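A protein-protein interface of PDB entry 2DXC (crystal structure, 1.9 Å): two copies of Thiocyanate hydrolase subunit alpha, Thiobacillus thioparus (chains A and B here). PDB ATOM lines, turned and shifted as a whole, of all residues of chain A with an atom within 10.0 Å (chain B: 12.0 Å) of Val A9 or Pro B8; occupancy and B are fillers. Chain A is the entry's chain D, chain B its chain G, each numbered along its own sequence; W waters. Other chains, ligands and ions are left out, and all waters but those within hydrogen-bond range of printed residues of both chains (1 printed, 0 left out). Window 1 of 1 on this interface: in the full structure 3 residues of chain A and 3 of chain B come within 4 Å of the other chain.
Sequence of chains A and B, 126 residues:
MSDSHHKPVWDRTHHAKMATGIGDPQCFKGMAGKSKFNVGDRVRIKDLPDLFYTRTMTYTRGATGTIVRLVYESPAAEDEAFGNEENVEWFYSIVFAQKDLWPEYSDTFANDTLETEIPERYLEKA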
ATOM      1  N   PRO A   8       5.953  12.495  -6.675  1.00  0.00           N
ATOM      2  CA  PRO A   8       5.945  11.337  -5.750  1.00  0.00           C
ATOM      3  C   PRO A   8       4.539  10.756  -5.642  1.00  0.00           C
ATOM      4  O   PRO A   8       3.564  11.497  -5.515  1.00  0.00           O
ATOM      5  CB  PRO A   8       6.421  11.848  -4.398  1.00  0.00           C
ATOM      6  CG  PRO A   8       5.977  13.308  -4.467  1.00  0.00           C
ATOM      7  CD  PRO A   8       6.251  13.728  -5.923  1.00  0.00           C
ATOM      8  N   VAL A   9       4.445   9.431  -5.698  1.00  0.00           N
ATOM      9  CA  VAL A   9       3.160   8.745  -5.609  1.00  0.00           C
ATOM     10  C   VAL A   9       3.111   7.863  -4.371  1.00  0.00           C
ATOM     11  O   VAL A   9       4.040   7.098  -4.108  1.00  0.00           O
ATOM     12  CB  VAL A   9       2.908   7.855  -6.849  1.00  0.00           C
ATOM     13  CG1 VAL A   9       1.595   7.096  -6.691  1.00  0.00           C
ATOM     14  CG2 VAL A   9       2.876   8.712  -8.106  1.00  0.00           C
ATOM     15  N   TRP A  10       2.025   7.973  -3.612  1.00  0.00           N
ATOM     16  CA  TRP A  10       1.860   7.168  -2.408  1.00  0.00           C
ATOM     17  C   TRP A  10       0.912   6.002  -2.660  1.00  0.00           C
ATOM     18  O   TRP A  10      -0.190   6.182  -3.183  1.00  0.00           O
ATOM     19  CB  TRP A  10       1.335   8.031  -1.260  1.00  0.00           C
ATOM     20  CG  TRP A  10       2.168   9.245  -1.031  1.00  0.00           C
ATOM     21  CD1 TRP A  10       2.129  10.410  -1.739  1.00  0.00           C
ATOM     22  CD2 TRP A  10       3.212   9.393  -0.065  1.00  0.00           C
ATOM     23  NE1 TRP A  10       3.088  11.277  -1.278  1.00  0.00           N
ATOM     24  CE2 TRP A  10       3.767  10.680  -0.251  1.00  0.00           C
ATOM     25  CE3 TRP A  10       3.735   8.566   0.938  1.00  0.00           C
ATOM     26  CZ2 TRP A  10       4.822  11.159   0.530  1.00  0.00           C
ATOM     27  CZ3 TRP A  10       4.785   9.043   1.717  1.00  0.00           C
ATOM     28  CH2 TRP A  10       5.317  10.330   1.507  1.00  0.00           C
ATOM     29  N   ASP A  11       1.348   4.805  -2.289  1.00  0.00           N
ATOM     30  CA  ASP A  11       0.545   3.605  -2.471  1.00  0.00           C
ATOM     31  C   ASP A  11      -0.568   3.561  -1.421  1.00  0.00           C
ATOM     32  O   ASP A  11      -0.321   3.242  -0.257  1.00  0.00           O
ATOM     33  CB  ASP A  11       1.424   2.364  -2.331  1.00  0.00           C
ATOM     34  CG  ASP A  11       0.765   1.120  -2.886  1.00  0.00           C
ATOM     35  OD1 ASP A  11      -0.476   1.017  -2.797  1.00  0.00           O
ATOM     36  OD2 ASP A  11       1.489   0.241  -3.401  1.00  0.00           O
ATOM     37  N   ARG A  12      -1.792   3.873  -1.835  1.00  0.00           N
ATOM     38  CA  ARG A  12      -2.921   3.878  -0.912  1.00  0.00           C
ATOM     39  C   ARG A  12      -3.670   2.553  -0.808  1.00  0.00           C
ATOM     40  O   ARG A  12      -4.674   2.463  -0.096  1.00  0.00           O
ATOM     41  CB  ARG A  12      -3.912   4.974  -1.306  1.00  0.00           C
ATOM     42  CG  ARG A  12      -3.482   6.380  -0.921  1.00  0.00           C
ATOM     43  CD  ARG A  12      -4.584   7.370  -1.237  1.00  0.00           C
ATOM     44  NE  ARG A  12      -4.634   7.698  -2.658  1.00  0.00           N
ATOM     45  CZ  ARG A  12      -5.705   8.188  -3.273  1.00  0.00           C
ATOM     46  NH1 ARG A  12      -6.823   8.400  -2.595  1.00  0.00           N
ATOM     47  NH2 ARG A  12      -5.651   8.486  -4.563  1.00  0.00           N
ATOM     48  N   THR A  13      -3.193   1.525  -1.505  1.00  0.00           N
ATOM     49  CA  THR A  13      -3.859   0.229  -1.463  1.00  0.00           C
ATOM     50  C   THR A  13      -3.032  -0.851  -0.772  1.00  0.00           C
ATOM     51  O   THR A  13      -3.556  -1.906  -0.423  1.00  0.00           O
ATOM     52  CB  THR A  13      -4.201  -0.276  -2.884  1.00  0.00           C
ATOM     53  OG1 THR A  13      -2.988  -0.504  -3.613  1.00  0.00           O
ATOM     54  CG2 THR A  13      -5.050   0.746  -3.628  1.00  0.00           C
ATOM     55  N   HIS A  14      -1.746  -0.587  -0.572  1.00  0.00           N
ATOM     56  CA  HIS A  14      -0.859  -1.563   0.052  1.00  0.00           C
ATOM     57  C   HIS A  14      -1.352  -2.159   1.370  1.00  0.00           C
ATOM     58  O   HIS A  14      -1.494  -3.373   1.485  1.00  0.00           O
ATOM     59  CB  HIS A  14       0.529  -0.960   0.279  1.00  0.00           C
ATOM     60  CG  HIS A  14       1.464  -1.875   1.005  1.00  0.00           C
ATOM     61  ND1 HIS A  14       1.944  -3.043   0.452  1.00  0.00           N
ATOM     62  CD2 HIS A  14       1.972  -1.817   2.260  1.00  0.00           C
ATOM     63  CE1 HIS A  14       2.706  -3.665   1.334  1.00  0.00           C
ATOM     64  NE2 HIS A  14       2.738  -2.942   2.439  1.00  0.00           N
ATOM     65  N   PHE A  82       6.861   6.297   9.968  1.00  0.00           N
ATOM     66  CA  PHE A  82       7.487   7.054   8.882  1.00  0.00           C
ATOM     67  C   PHE A  82       7.339   6.333   7.545  1.00  0.00           C
ATOM     68  O   PHE A  82       8.033   6.640   6.575  1.00  0.00           O
ATOM     69  CB  PHE A  82       8.962   7.330   9.204  1.00  0.00           C
ATOM     70  CG  PHE A  82       9.151   8.393  10.251  1.00  0.00           C
ATOM     71  CD1 PHE A  82       9.045   9.742   9.919  1.00  0.00           C
ATOM     72  CD2 PHE A  82       9.362   8.047  11.581  1.00  0.00           C
ATOM     73  CE1 PHE A  82       9.139  10.731  10.900  1.00  0.00           C
ATOM     74  CE2 PHE A  82       9.457   9.029  12.570  1.00  0.00           C
ATOM     75  CZ  PHE A  82       9.345  10.371  12.229  1.00  0.00           C
ATOM     76  N   GLY A  83       6.418   5.372   7.509  1.00  0.00           N
ATOM     77  CA  GLY A  83       6.143   4.633   6.286  1.00  0.00           C
ATOM     78  C   GLY A  83       7.122   3.535   5.932  1.00  0.00           C
ATOM     79  O   GLY A  83       7.154   3.080   4.790  1.00  0.00           O
ATOM     80  N   ASN A  84       7.919   3.103   6.902  1.00  0.00           N
ATOM     81  CA  ASN A  84       8.903   2.051   6.668  1.00  0.00           C
ATOM     82  C   ASN A  84       8.433   0.769   7.357  1.00  0.00           C
ATOM     83  O   ASN A  84       8.527   0.646   8.578  1.00  0.00           O
ATOM     84  CB  ASN A  84      10.262   2.488   7.228  1.00  0.00           C
ATOM     85  CG  ASN A  84      10.692   3.857   6.716  1.00  0.00           C
ATOM     86  OD1 ASN A  84      11.168   4.704   7.483  1.00  0.00           O
ATOM     87  ND2 ASN A  84      10.530   4.079   5.417  1.00  0.00           N
ATOM     88  N   LYS B   7       7.924   3.420  -1.293  1.00  0.00           N
ATOM     89  CA  LYS B   7       7.525   3.540  -2.724  1.00  0.00           C
ATOM     90  C   LYS B   7       7.793   4.928  -3.300  1.00  0.00           C
ATOM     91  O   LYS B   7       8.360   5.052  -4.386  1.00  0.00           O
ATOM     92  CB  LYS B   7       6.037   3.215  -2.899  1.00  0.00           C
ATOM     93  CG  LYS B   7       5.668   1.775  -2.627  1.00  0.00           C
ATOM     94  CD  LYS B   7       6.391   0.826  -3.567  1.00  0.00           C
ATOM     95  CE  LYS B   7       5.990  -0.614  -3.290  1.00  0.00           C
ATOM     96  NZ  LYS B   7       6.198  -0.975  -1.858  1.00  0.00           N
ATOM     97  N   PRO B   8       7.389   5.991  -2.583  1.00  0.00           N
ATOM     98  CA  PRO B   8       7.607   7.355  -3.074  1.00  0.00           C
ATOM     99  C   PRO B   8       9.039   7.613  -3.529  1.00  0.00           C
ATOM    100  O   PRO B   8       9.993   7.329  -2.802  1.00  0.00           O
ATOM    101  CB  PRO B   8       7.223   8.219  -1.875  1.00  0.00           C
ATOM    102  CG  PRO B   8       6.176   7.402  -1.192  1.00  0.00           C
ATOM    103  CD  PRO B   8       6.772   6.014  -1.244  1.00  0.00           C
ATOM    104  N   VAL B   9       9.176   8.144  -4.738  1.00  0.00           N
ATOM    105  CA  VAL B   9      10.480   8.473  -5.300  1.00  0.00           C
ATOM    106  C   VAL B   9      10.540   9.983  -5.488  1.00  0.00           C
ATOM    107  O   VAL B   9       9.663  10.573  -6.123  1.00  0.00           O
ATOM    108  CB  VAL B   9      10.697   7.802  -6.672  1.00  0.00           C
ATOM    109  CG1 VAL B   9      11.986   8.316  -7.308  1.00  0.00           C
ATOM    110  CG2 VAL B   9      10.754   6.292  -6.505  1.00  0.00           C
ATOM    111  N   TRP B  10      11.570  10.608  -4.928  1.00  0.00           N
ATOM    112  CA  TRP B  10      11.721  12.050  -5.046  1.00  0.00           C
ATOM    113  C   TRP B  10      12.692  12.409  -6.160  1.00  0.00           C
ATOM    114  O   TRP B  10      13.812  11.901  -6.209  1.00  0.00           O
ATOM    115  CB  TRP B  10      12.202  12.641  -3.721  1.00  0.00           C
ATOM    116  CG  TRP B  10      11.329  12.255  -2.576  1.00  0.00           C
ATOM    117  CD1 TRP B  10      11.398  11.106  -1.839  1.00  0.00           C
ATOM    118  CD2 TRP B  10      10.203  12.984  -2.077  1.00  0.00           C
ATOM    119  NE1 TRP B  10      10.384  11.073  -0.914  1.00  0.00           N
ATOM    120  CE2 TRP B  10       9.634  12.213  -1.039  1.00  0.00           C
ATOM    121  CE3 TRP B  10       9.618  14.214  -2.408  1.00  0.00           C
ATOM    122  CZ2 TRP B  10       8.508  12.631  -0.328  1.00  0.00           C
ATOM    123  CZ3 TRP B  10       8.495  14.631  -1.698  1.00  0.00           C
ATOM    124  CH2 TRP B  10       7.954  13.840  -0.671  1.00  0.00           C
ATOM    125  N   ASP B  11      12.247  13.281  -7.057  1.00  0.00           N
ATOM    126  CA  ASP B  11      13.074  13.723  -8.168  1.00  0.00           C
ATOM    127  C   ASP B  11      14.083  14.731  -7.630  1.00  0.00           C
ATOM    128  O   ASP B  11      13.729  15.871  -7.329  1.00  0.00           O
ATOM    129  CB  ASP B  11      12.213  14.395  -9.239  1.00  0.00           C
ATOM    130  CG  ASP B  11      13.003  14.740 -10.484  1.00  0.00           C
ATOM    131  OD1 ASP B  11      14.234  14.923 -10.373  1.00  0.00           O
ATOM    132  OD2 ASP B  11      12.393  14.842 -11.570  1.00  0.00           O
ATOM    133  N   ARG B  12      15.337  14.310  -7.516  1.00  0.00           N
ATOM    134  CA  ARG B  12      16.381  15.183  -7.003  1.00  0.00           C
ATOM    135  C   ARG B  12      17.115  15.988  -8.072  1.00  0.00           C
ATOM    136  O   ARG B  12      18.043  16.729  -7.754  1.00  0.00           O
ATOM    137  CB  ARG B  12      17.399  14.364  -6.208  1.00  0.00           C
ATOM    138  CG  ARG B  12      16.928  13.956  -4.821  1.00  0.00           C
ATOM    139  CD  ARG B  12      18.006  13.158  -4.113  1.00  0.00           C
ATOM    140  NE  ARG B  12      17.905  11.731  -4.394  1.00  0.00           N
ATOM    141  CZ  ARG B  12      18.931  10.887  -4.355  1.00  0.00           C
ATOM    142  NH1 ARG B  12      20.147  11.329  -4.058  1.00  0.00           N
ATOM    143  NH2 ARG B  12      18.737   9.596  -4.595  1.00  0.00           N
ATOM    144  N   PHE B  82       6.215  23.291   0.104  1.00  0.00           N
ATOM    145  CA  PHE B  82       5.621  21.963   0.194  1.00  0.00           C
ATOM    146  C   PHE B  82       5.824  21.170  -1.093  1.00  0.00           C
ATOM    147  O   PHE B  82       5.102  20.209  -1.368  1.00  0.00           O
ATOM    148  CB  PHE B  82       4.135  22.075   0.552  1.00  0.00           C
ATOM    149  CG  PHE B  82       3.897  22.423   1.999  1.00  0.00           C
ATOM    150  CD1 PHE B  82       3.958  21.441   2.985  1.00  0.00           C
ATOM    151  CD2 PHE B  82       3.663  23.740   2.384  1.00  0.00           C
ATOM    152  CE1 PHE B  82       3.789  21.767   4.333  1.00  0.00           C
ATOM    153  CE2 PHE B  82       3.494  24.077   3.726  1.00  0.00           C
ATOM    154  CZ  PHE B  82       3.557  23.090   4.703  1.00  0.00           C
ATOM    155  N   GLY B  83       6.821  21.581  -1.873  1.00  0.00           N
ATOM    156  CA  GLY B  83       7.146  20.897  -3.113  1.00  0.00           C
ATOM    157  C   GLY B  83       6.195  21.093  -4.283  1.00  0.00           C
ATOM    158  O   GLY B  83       6.216  20.309  -5.233  1.00  0.00           O
ATOM    159  N   ASN B  84       5.369  22.134  -4.231  1.00  0.00           N
ATOM    160  CA  ASN B  84       4.413  22.398  -5.306  1.00  0.00           C
ATOM    161  C   ASN B  84       4.850  23.636  -6.085  1.00  0.00           C
ATOM    162  O   ASN B  84       4.631  24.760  -5.638  1.00  0.00           O
ATOM    163  CB  ASN B  84       3.013  22.623  -4.719  1.00  0.00           C
ATOM    164  CG  ASN B  84       2.576  21.493  -3.794  1.00  0.00           C
ATOM    165  OD1 ASN B  84       2.125  21.736  -2.670  1.00  0.00           O
ATOM    166  ND2 ASN B  84       2.697  20.254  -4.263  1.00  0.00           N
HETATM  167  O   HOH W   1       6.853   7.955  -6.428  1.00  0.00           O
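Pro A8 touches Val B9 (CA to O, 3.8 Å).
Pro A8 touches Trp B10 (CG to CZ3, 3.97 Å).
CG of Pro B8 touches O of Val A9 (3.6 Å).
CG of Pro B8 touches CE3 of Trp A10 (3.4 Å).
Val A9 touches one residue of chain B.
Of chain A, only Val A9 (3.6 Å) and Trp A10 (3.4 Å) come within 4 Å of Pro B8.
Trp A10 touches just one residue of chain B: Pro B8.
Printed residues of chain A within 4 Å of Val B9: Pro A8 (3.8 Å).
Of the printed residues of chain A, Trp B10 touches Pro A8 (3.97 Å).
Phe A82 touches none of the printed residues of chain B.
Arg A12 touches none of the printed residues of chain B.
The nearest residue of chain B that does not touch Val A9 is Lys B7 (4.4 Å).
The nearest residue of chain A that does not touch Pro B8 is Pro A8 (4.5 Å).
Hydrophobic or aromatic side chains of chain A that line the printed part of chain B: Pro A8 and Trp A10.
Of the 9 printed residues of chain B, 3 touch a printed residue of chain A.
Hydrophobic or aromatic side chains of chain B within 4 Å of the printed part of chain A: Pro B8 and Trp B10.
Among the printed residues, 4 pairs touch across the chains.
Among the printed residues, no Asp or Glu carboxylate lies within 4 Å of a Lys or Arg side-chain nitrogen of the other chain.
Pro A8 touches Val B9, and with the chains exchanged Val A9 touches Pro B8.
Pro A8 touches Trp B10, and with the chains exchanged Trp A10 touches Pro B8.
8 positions are printed for both chains.
Water W1 bridges N of Val B9 and N of Val A9.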
